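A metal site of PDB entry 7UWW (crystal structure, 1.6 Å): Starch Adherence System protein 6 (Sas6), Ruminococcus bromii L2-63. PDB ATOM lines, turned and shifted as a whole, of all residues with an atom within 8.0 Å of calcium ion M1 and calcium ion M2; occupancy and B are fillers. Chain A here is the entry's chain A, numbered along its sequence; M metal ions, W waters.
The side-chain carboxylate (OE2) of Glu 525 sits close to the backbone NH (N) of Gln 511. OG of Ser 523 lies close to N of Glu 525, 3.1 Å away. The side-chain hydroxyl (OG) of Ser 507 is in hydrogen-bond range of the backbone NH (N) of Asn 531 (3.3 Å). N of Ser 507 lies within hydrogen-bond range of OD1 of Asp 505, 2.8 Å away. The side-chain amide nitrogen (NE2) of Gln 511 lies close to the side-chain carboxylate (OD2) of Asp 528 (3.1 Å). O of Asp 528 lies within hydrogen-bond range of N of Gly 354 (3.3 Å). O of Gly 354 sits at hydrogen-bond distance from N of Asp 530 (3.0 Å). N of Gly 498 is in hydrogen-bond range of OG1 of Thr 355, at 3.3 Å.
Calcium ion M1 is bound by the side-chain carboxylate (OD1) of Asp 510, the backbone carbonyl oxygen (O) of Ser 507, the side-chain carboxylate (OD2) of Asp 528, the side-chain carboxylate (OD1) of Asp 530, water W1, the side-chain carboxylate (OE2) of Glu 525 and the side-chain carboxylate (OE1) of Glu 525.
Calcium ion M2 is bound by OE1 of Glu 525 (2.2 Å), OD2 of Asp 530 (2.4 Å), OG of Ser 497 (2.4 Å), O of Gly 498 (2.4 Å), OD1 of Asp 528 (2.4 Å), O of Glu 525 (2.4 Å) and OD1 of Asp 530 (2.6 Å).
Water W1 lies within hydrogen-bond range of the side-chain carboxylate (OD2) of Asp 510 and the backbone carbonyl oxygen (O) of Ile 529.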
ATOM      1  N   PRO A 250     -26.875  24.875  15.517  1.00  0.00           N
ATOM      2  CA  PRO A 250     -28.220  24.271  15.432  1.00  0.00           C
ATOM      3  C   PRO A 250     -29.113  24.531  16.631  1.00  0.00           C
ATOM      4  O   PRO A 250     -30.342  24.547  16.480  1.00  0.00           O
ATOM      5  CB  PRO A 250     -27.929  22.768  15.283  1.00  0.00           C
ATOM      6  CG  PRO A 250     -26.566  22.715  14.541  1.00  0.00           C
ATOM      7  CD  PRO A 250     -25.788  23.899  15.213  1.00  0.00           C
ATOM      8  N   GLY A 353     -24.229   9.587  13.761  1.00  0.00           N
ATOM      9  CA  GLY A 353     -23.927  10.874  13.176  1.00  0.00           C
ATOM     10  C   GLY A 353     -22.537  10.939  12.586  1.00  0.00           C
ATOM     11  O   GLY A 353     -21.597  10.286  13.065  1.00  0.00           O
ATOM     12  N   GLY A 354     -22.414  11.750  11.542  1.00  0.00           N
ATOM     13  CA  GLY A 354     -21.136  12.026  10.922  1.00  0.00           C
ATOM     14  C   GLY A 354     -21.349  12.987   9.783  1.00  0.00           C
ATOM     15  O   GLY A 354     -22.477  13.431   9.496  1.00  0.00           O
ATOM     16  N   THR A 355     -20.247  13.334   9.117  1.00  0.00           N
ATOM     17  CA  THR A 355     -20.288  14.251   7.985  1.00  0.00           C
ATOM     18  C   THR A 355     -19.614  13.563   6.813  1.00  0.00           C
ATOM     19  O   THR A 355     -18.448  13.151   6.938  1.00  0.00           O
ATOM     20  CB  THR A 355     -19.558  15.561   8.324  1.00  0.00           C
ATOM     21  OG1 THR A 355     -20.112  16.163   9.522  1.00  0.00           O
ATOM     22  CG2 THR A 355     -19.647  16.535   7.142  1.00  0.00           C
ATOM     23  N   LEU A 492     -16.922  21.457  12.955  1.00  0.00           N
ATOM     24  CA  LEU A 492     -17.179  21.339  14.382  1.00  0.00           C
ATOM     25  C   LEU A 492     -18.289  20.314  14.588  1.00  0.00           C
ATOM     26  O   LEU A 492     -19.248  20.248  13.810  1.00  0.00           O
ATOM     27  CB  LEU A 492     -17.619  22.670  14.991  1.00  0.00           C
ATOM     28  CG  LEU A 492     -16.679  23.853  14.998  1.00  0.00           C
ATOM     29  CD1 LEU A 492     -17.287  24.966  15.809  1.00  0.00           C
ATOM     30  CD2 LEU A 492     -15.351  23.417  15.545  1.00  0.00           C
ATOM     31  N   THR A 493     -18.134  19.505  15.641  1.00  0.00           N
ATOM     32  CA  THR A 493     -19.133  18.529  16.058  1.00  0.00           C
ATOM     33  C   THR A 493     -19.533  18.772  17.521  1.00  0.00           C
ATOM     34  O   THR A 493     -18.941  19.598  18.227  1.00  0.00           O
ATOM     35  CB  THR A 493     -18.598  17.091  15.926  1.00  0.00           C
ATOM     36  OG1 THR A 493     -17.764  16.815  17.072  1.00  0.00           O
ATOM     37  CG2 THR A 493     -17.869  16.868  14.585  1.00  0.00           C
ATOM     38  N   TYR A 494     -20.540  18.023  17.959  1.00  0.00           N
ATOM     39  CA  TYR A 494     -20.776  17.846  19.379  1.00  0.00           C
ATOM     40  C   TYR A 494     -20.609  16.377  19.733  1.00  0.00           C
ATOM     41  O   TYR A 494     -21.379  15.796  20.507  1.00  0.00           O
ATOM     42  CB  TYR A 494     -22.148  18.365  19.791  1.00  0.00           C
ATOM     43  CG  TYR A 494     -22.322  18.661  21.268  1.00  0.00           C
ATOM     44  CD1 TYR A 494     -21.375  18.297  22.189  1.00  0.00           C
ATOM     45  CD2 TYR A 494     -23.466  19.287  21.721  1.00  0.00           C
ATOM     46  CE1 TYR A 494     -21.540  18.552  23.540  1.00  0.00           C
ATOM     47  CE2 TYR A 494     -23.649  19.557  23.080  1.00  0.00           C
ATOM     48  CZ  TYR A 494     -22.676  19.183  23.990  1.00  0.00           C
ATOM     49  OH  TYR A 494     -22.849  19.436  25.352  1.00  0.00           O
ATOM     50  N   THR A 496     -20.128  13.634  17.234  1.00  0.00           N
ATOM     51  CA  THR A 496     -20.239  12.784  16.062  1.00  0.00           C
ATOM     52  C   THR A 496     -20.589  13.612  14.813  1.00  0.00           C
ATOM     53  O   THR A 496     -19.707  13.973  14.020  1.00  0.00           O
ATOM     54  CB  THR A 496     -21.296  11.700  16.287  1.00  0.00           C
ATOM     55  OG1 THR A 496     -22.521  12.290  16.762  1.00  0.00           O
ATOM     56  CG2 THR A 496     -20.775  10.675  17.291  1.00  0.00           C
ATOM     57  N   SER A 497     -21.875  13.957  14.684  1.00  0.00           N
ATOM     58  CA  SER A 497     -22.374  14.758  13.560  1.00  0.00           C
ATOM     59  C   SER A 497     -21.810  16.165  13.563  1.00  0.00           C
ATOM     60  O   SER A 497     -21.524  16.757  14.613  1.00  0.00           O
ATOM     61  CB  SER A 497     -23.909  14.828  13.609  1.00  0.00           C
ATOM     62  OG  SER A 497     -24.416  15.364  12.383  1.00  0.00           O
ATOM     63  N   GLY A 498     -21.740  16.748  12.381  1.00  0.00           N
ATOM     64  CA  GLY A 498     -21.388  18.157  12.289  1.00  0.00           C
ATOM     65  C   GLY A 498     -22.457  19.039  12.889  1.00  0.00           C
ATOM     66  O   GLY A 498     -23.631  18.671  12.953  1.00  0.00           O
ATOM     67  N   MET A 499     -22.010  20.182  13.393  1.00  0.00           N
ATOM     68  CA  MET A 499     -22.847  21.265  13.923  1.00  0.00           C
ATOM     69  C   MET A 499     -22.668  22.578  13.191  1.00  0.00           C
ATOM     70  O   MET A 499     -23.626  23.322  13.015  1.00  0.00           O
ATOM     71  CB  MET A 499     -22.500  21.452  15.391  1.00  0.00           C
ATOM     72  CG  MET A 499     -22.803  20.239  16.260  1.00  0.00           C
ATOM     73  SD  MET A 499     -24.557  19.927  16.460  1.00  0.00           S
ATOM     74  CE  MET A 499     -24.891  21.066  17.831  1.00  0.00           C
ATOM     75  N   ASP A 500     -21.450  22.899  12.767  1.00  0.00           N
ATOM     76  CA  ASP A 500     -21.107  24.149  12.091  1.00  0.00           C
ATOM     77  C   ASP A 500     -19.865  23.845  11.260  1.00  0.00           C
ATOM     78  O   ASP A 500     -19.083  22.972  11.626  1.00  0.00           O
ATOM     79  CB  ASP A 500     -20.901  25.280  13.139  1.00  0.00           C
ATOM     80  CG  ASP A 500     -20.982  26.680  12.550  1.00  0.00           C
ATOM     81  OD1 ASP A 500     -21.021  26.832  11.317  1.00  0.00           O
ATOM     82  OD2 ASP A 500     -20.978  27.669  13.343  1.00  0.00           O
ATOM     83  N   ASP A 505     -21.959  25.170   5.460  1.00  0.00           N
ATOM     84  CA  ASP A 505     -22.706  24.272   4.587  1.00  0.00           C
ATOM     85  C   ASP A 505     -24.127  24.077   5.102  1.00  0.00           C
ATOM     86  O   ASP A 505     -24.353  23.954   6.316  1.00  0.00           O
ATOM     87  CB  ASP A 505     -22.003  22.905   4.505  1.00  0.00           C
ATOM     88  CG  ASP A 505     -22.628  21.989   3.492  1.00  0.00           C
ATOM     89  OD1 ASP A 505     -23.710  21.415   3.757  1.00  0.00           O
ATOM     90  OD2 ASP A 505     -22.074  21.872   2.369  1.00  0.00           O
ATOM     91  N   PRO A 506     -25.127  24.123   4.215  1.00  0.00           N
ATOM     92  CA  PRO A 506     -26.529  24.052   4.682  1.00  0.00           C
ATOM     93  C   PRO A 506     -26.885  22.728   5.328  1.00  0.00           C
ATOM     94  O   PRO A 506     -27.909  22.656   6.030  1.00  0.00           O
ATOM     95  CB  PRO A 506     -27.350  24.311   3.392  1.00  0.00           C
ATOM     96  CG  PRO A 506     -26.467  23.857   2.291  1.00  0.00           C
ATOM     97  CD  PRO A 506     -25.047  24.248   2.740  1.00  0.00           C
ATOM     98  N   SER A 507     -26.097  21.660   5.127  1.00  0.00           N
ATOM     99  CA  SER A 507     -26.427  20.431   5.805  1.00  0.00           C
ATOM    100  C   SER A 507     -26.215  20.562   7.311  1.00  0.00           C
ATOM    101  O   SER A 507     -26.629  19.688   8.050  1.00  0.00           O
ATOM    102  CB  SER A 507     -25.636  19.231   5.253  1.00  0.00           C
ATOM    103  OG  SER A 507     -24.257  19.344   5.512  1.00  0.00           O
ATOM    104  N   MET A 508     -25.593  21.656   7.780  1.00  0.00           N
ATOM    105  CA  MET A 508     -25.439  21.810   9.225  1.00  0.00           C
ATOM    106  C   MET A 508     -26.771  22.195   9.889  1.00  0.00           C
ATOM    107  O   MET A 508     -26.903  22.062  11.112  1.00  0.00           O
ATOM    108  CB  MET A 508     -24.375  22.852   9.546  1.00  0.00           C
ATOM    109  CG  MET A 508     -22.957  22.521   9.137  1.00  0.00           C
ATOM    110  SD  MET A 508     -22.368  21.041   9.922  1.00  0.00           S
ATOM    111  CE  MET A 508     -22.348  19.945   8.514  1.00  0.00           C
ATOM    112  N   LEU A 509     -27.724  22.664   9.107  1.00  0.00           N
ATOM    113  CA  LEU A 509     -28.984  23.214   9.620  1.00  0.00           C
ATOM    114  C   LEU A 509     -30.227  22.601   8.975  1.00  0.00           C
ATOM    115  O   LEU A 509     -31.332  23.005   9.327  1.00  0.00           O
ATOM    116  CB  LEU A 509     -29.005  24.722   9.421  1.00  0.00           C
ATOM    117  CG  LEU A 509     -27.935  25.486  10.260  1.00  0.00           C
ATOM    118  CD1 LEU A 509     -27.984  26.969   9.885  1.00  0.00           C
ATOM    119  CD2 LEU A 509     -28.143  25.321  11.714  1.00  0.00           C
ATOM    120  N   ASP A 510     -30.066  21.637   8.065  1.00  0.00           N
ATOM    121  CA  ASP A 510     -31.214  21.108   7.341  1.00  0.00           C
ATOM    122  C   ASP A 510     -32.197  20.388   8.250  1.00  0.00           C
ATOM    123  O   ASP A 510     -33.384  20.313   7.908  1.00  0.00           O
ATOM    124  CB  ASP A 510     -30.748  20.235   6.159  1.00  0.00           C
ATOM    125  CG  ASP A 510     -29.997  18.951   6.570  1.00  0.00           C
ATOM    126  OD1 ASP A 510     -29.500  18.824   7.695  1.00  0.00           O
ATOM    127  OD2 ASP A 510     -29.881  18.052   5.713  1.00  0.00           O
ATOM    128  N   GLN A 511     -31.756  19.922   9.436  1.00  0.00           N
ATOM    129  CA  GLN A 511     -32.594  19.252  10.435  1.00  0.00           C
ATOM    130  C   GLN A 511     -32.417  19.882  11.817  1.00  0.00           C
ATOM    131  O   GLN A 511     -32.617  19.210  12.844  1.00  0.00           O
ATOM    132  CB  GLN A 511     -32.290  17.766  10.468  1.00  0.00           C
ATOM    133  CG  GLN A 511     -32.434  17.133   9.072  1.00  0.00           C
ATOM    134  CD  GLN A 511     -32.524  15.617   9.100  1.00  0.00           C
ATOM    135  OE1 GLN A 511     -33.558  15.048   8.810  1.00  0.00           O
ATOM    136  NE2 GLN A 511     -31.423  14.958   9.430  1.00  0.00           N
ATOM    137  N   ALA A 512     -32.110  21.178  11.868  1.00  0.00           N
ATOM    138  CA  ALA A 512     -31.765  21.812  13.139  1.00  0.00           C
ATOM    139  C   ALA A 512     -32.963  21.900  14.086  1.00  0.00           C
ATOM    140  O   ALA A 512     -32.798  21.817  15.312  1.00  0.00           O
ATOM    141  CB  ALA A 512     -31.224  23.210  12.906  1.00  0.00           C
ATOM    142  N   SER A 523     -31.122  19.577  19.618  1.00  0.00           N
ATOM    143  CA  SER A 523     -31.230  19.463  18.165  1.00  0.00           C
ATOM    144  C   SER A 523     -30.718  18.124  17.653  1.00  0.00           C
ATOM    145  O   SER A 523     -29.657  17.650  18.084  1.00  0.00           O
ATOM    146  CB  SER A 523     -30.453  20.582  17.470  1.00  0.00           C
ATOM    147  OG  SER A 523     -30.519  20.445  16.069  1.00  0.00           O
ATOM    148  N   HIS A 524     -31.496  17.535  16.730  1.00  0.00           N
ATOM    149  CA  HIS A 524     -31.158  16.342  15.983  1.00  0.00           C
ATOM    150  C   HIS A 524     -29.890  16.502  15.155  1.00  0.00           C
ATOM    151  O   HIS A 524     -29.301  15.497  14.747  1.00  0.00           O
ATOM    152  CB  HIS A 524     -32.348  16.006  15.074  1.00  0.00           C
ATOM    153  CG  HIS A 524     -32.190  14.757  14.266  1.00  0.00           C
ATOM    154  ND1 HIS A 524     -31.988  13.530  14.840  1.00  0.00           N
ATOM    155  CD2 HIS A 524     -32.232  14.549  12.923  1.00  0.00           C
ATOM    156  CE1 HIS A 524     -31.909  12.603  13.891  1.00  0.00           C
ATOM    157  NE2 HIS A 524     -32.039  13.201  12.715  1.00  0.00           N
ATOM    158  N   GLU A 525     -29.441  17.731  14.920  1.00  0.00           N
ATOM    159  CA  GLU A 525     -28.213  17.939  14.169  1.00  0.00           C
ATOM    160  C   GLU A 525     -27.001  17.360  14.879  1.00  0.00           C
ATOM    161  O   GLU A 525     -25.951  17.209  14.255  1.00  0.00           O
ATOM    162  CB  GLU A 525     -27.983  19.444  13.912  1.00  0.00           C
ATOM    163  CG  GLU A 525     -28.729  19.983  12.700  1.00  0.00           C
ATOM    164  CD  GLU A 525     -28.280  19.361  11.366  1.00  0.00           C
ATOM    165  OE1 GLU A 525     -27.181  18.724  11.354  1.00  0.00           O
ATOM    166  OE2 GLU A 525     -29.035  19.523  10.367  1.00  0.00           O
ATOM    167  N   LYS A 526     -27.114  17.072  16.174  1.00  0.00           N
ATOM    168  CA  LYS A 526     -26.021  16.443  16.906  1.00  0.00           C
ATOM    169  C   LYS A 526     -25.783  14.992  16.498  1.00  0.00           C
ATOM    170  O   LYS A 526     -24.712  14.462  16.786  1.00  0.00           O
ATOM    171  CB  LYS A 526     -26.334  16.486  18.422  1.00  0.00           C
ATOM    172  CG  LYS A 526     -26.414  17.867  19.003  1.00  0.00           C
ATOM    173  CD  LYS A 526     -26.528  17.823  20.524  1.00  0.00           C
ATOM    174  CE  LYS A 526     -27.910  17.356  20.993  1.00  0.00           C
ATOM    175  NZ  LYS A 526     -28.033  17.452  22.518  1.00  0.00           N
ATOM    176  N   GLU A 527     -26.747  14.363  15.826  1.00  0.00           N
ATOM    177  CA  GLU A 527     -26.695  12.937  15.565  1.00  0.00           C
ATOM    178  C   GLU A 527     -27.063  12.526  14.142  1.00  0.00           C
ATOM    179  O   GLU A 527     -27.089  11.324  13.863  1.00  0.00           O
ATOM    180  CB  GLU A 527     -27.649  12.214  16.555  1.00  0.00           C
ATOM    181  CG  GLU A 527     -29.132  12.426  16.200  1.00  0.00           C
ATOM    182  CD  GLU A 527     -30.107  11.868  17.241  1.00  0.00           C
ATOM    183  OE1 GLU A 527     -29.735  10.918  17.996  1.00  0.00           O
ATOM    184  OE2 GLU A 527     -31.262  12.363  17.270  1.00  0.00           O
ATOM    185  N   ASP A 528     -27.308  13.458  13.226  1.00  0.00           N
ATOM    186  CA  ASP A 528     -27.741  13.082  11.896  1.00  0.00           C
ATOM    187  C   ASP A 528     -26.541  12.938  10.964  1.00  0.00           C
ATOM    188  O   ASP A 528     -25.389  13.120  11.355  1.00  0.00           O
ATOM    189  CB  ASP A 528     -28.757  14.081  11.333  1.00  0.00           C
ATOM    190  CG  ASP A 528     -28.171  15.458  11.088  1.00  0.00           C
ATOM    191  OD1 ASP A 528     -27.201  15.830  11.789  1.00  0.00           O
ATOM    192  OD2 ASP A 528     -28.722  16.216  10.247  1.00  0.00           O
ATOM    193  N   ILE A 529     -26.818  12.603   9.705  1.00  0.00           N
ATOM    194  CA  ILE A 529     -25.779  12.460   8.692  1.00  0.00           C
ATOM    195  C   ILE A 529     -25.804  13.684   7.797  1.00  0.00           C
ATOM    196  O   ILE A 529     -26.801  13.991   7.141  1.00  0.00           O
ATOM    197  CB  ILE A 529     -25.955  11.153   7.899  1.00  0.00           C
ATOM    198  CG1 ILE A 529     -25.739   9.949   8.822  1.00  0.00           C
ATOM    199  CG2 ILE A 529     -24.940  11.085   6.722  1.00  0.00           C
ATOM    200  CD1 ILE A 529     -25.773   8.603   8.101  1.00  0.00           C
ATOM    201  N   ASP A 530     -24.711  14.439   7.827  1.00  0.00           N
ATOM    202  CA  ASP A 530     -24.534  15.665   7.078  1.00  0.00           C
ATOM    203  C   ASP A 530     -23.773  15.271   5.822  1.00  0.00           C
ATOM    204  O   ASP A 530     -23.152  14.211   5.792  1.00  0.00           O
ATOM    205  CB  ASP A 530     -23.777  16.714   7.886  1.00  0.00           C
ATOM    206  CG  ASP A 530     -24.460  17.064   9.227  1.00  0.00           C
ATOM    207  OD1 ASP A 530     -25.714  17.045   9.310  1.00  0.00           O
ATOM    208  OD2 ASP A 530     -23.718  17.328  10.224  1.00  0.00           O
ATOM    209  N   ASN A 531     -23.857  16.096   4.796  1.00  0.00           N
ATOM    210  CA  ASN A 531     -23.136  15.801   3.560  1.00  0.00           C
ATOM    211  C   ASN A 531     -22.755  17.114   2.892  1.00  0.00           C
ATOM    212  O   ASN A 531     -23.611  17.918   2.547  1.00  0.00           O
ATOM    213  CB  ASN A 531     -23.967  14.944   2.615  1.00  0.00           C
ATOM    214  CG  ASN A 531     -23.180  14.537   1.380  1.00  0.00           C
ATOM    215  OD1 ASN A 531     -23.119  15.272   0.409  1.00  0.00           O
ATOM    216  ND2 ASN A 531     -22.526  13.368   1.438  1.00  0.00           N
HETATM  217 CA    CA M   1     -27.843  17.952   8.985  1.00  0.00          CA
HETATM  218 CA    CA M   2     -25.410  17.475  11.882  1.00  0.00          CA
HETATM  219  O   HOH W   1     -28.070  16.572   7.034  1.00  0.00           O
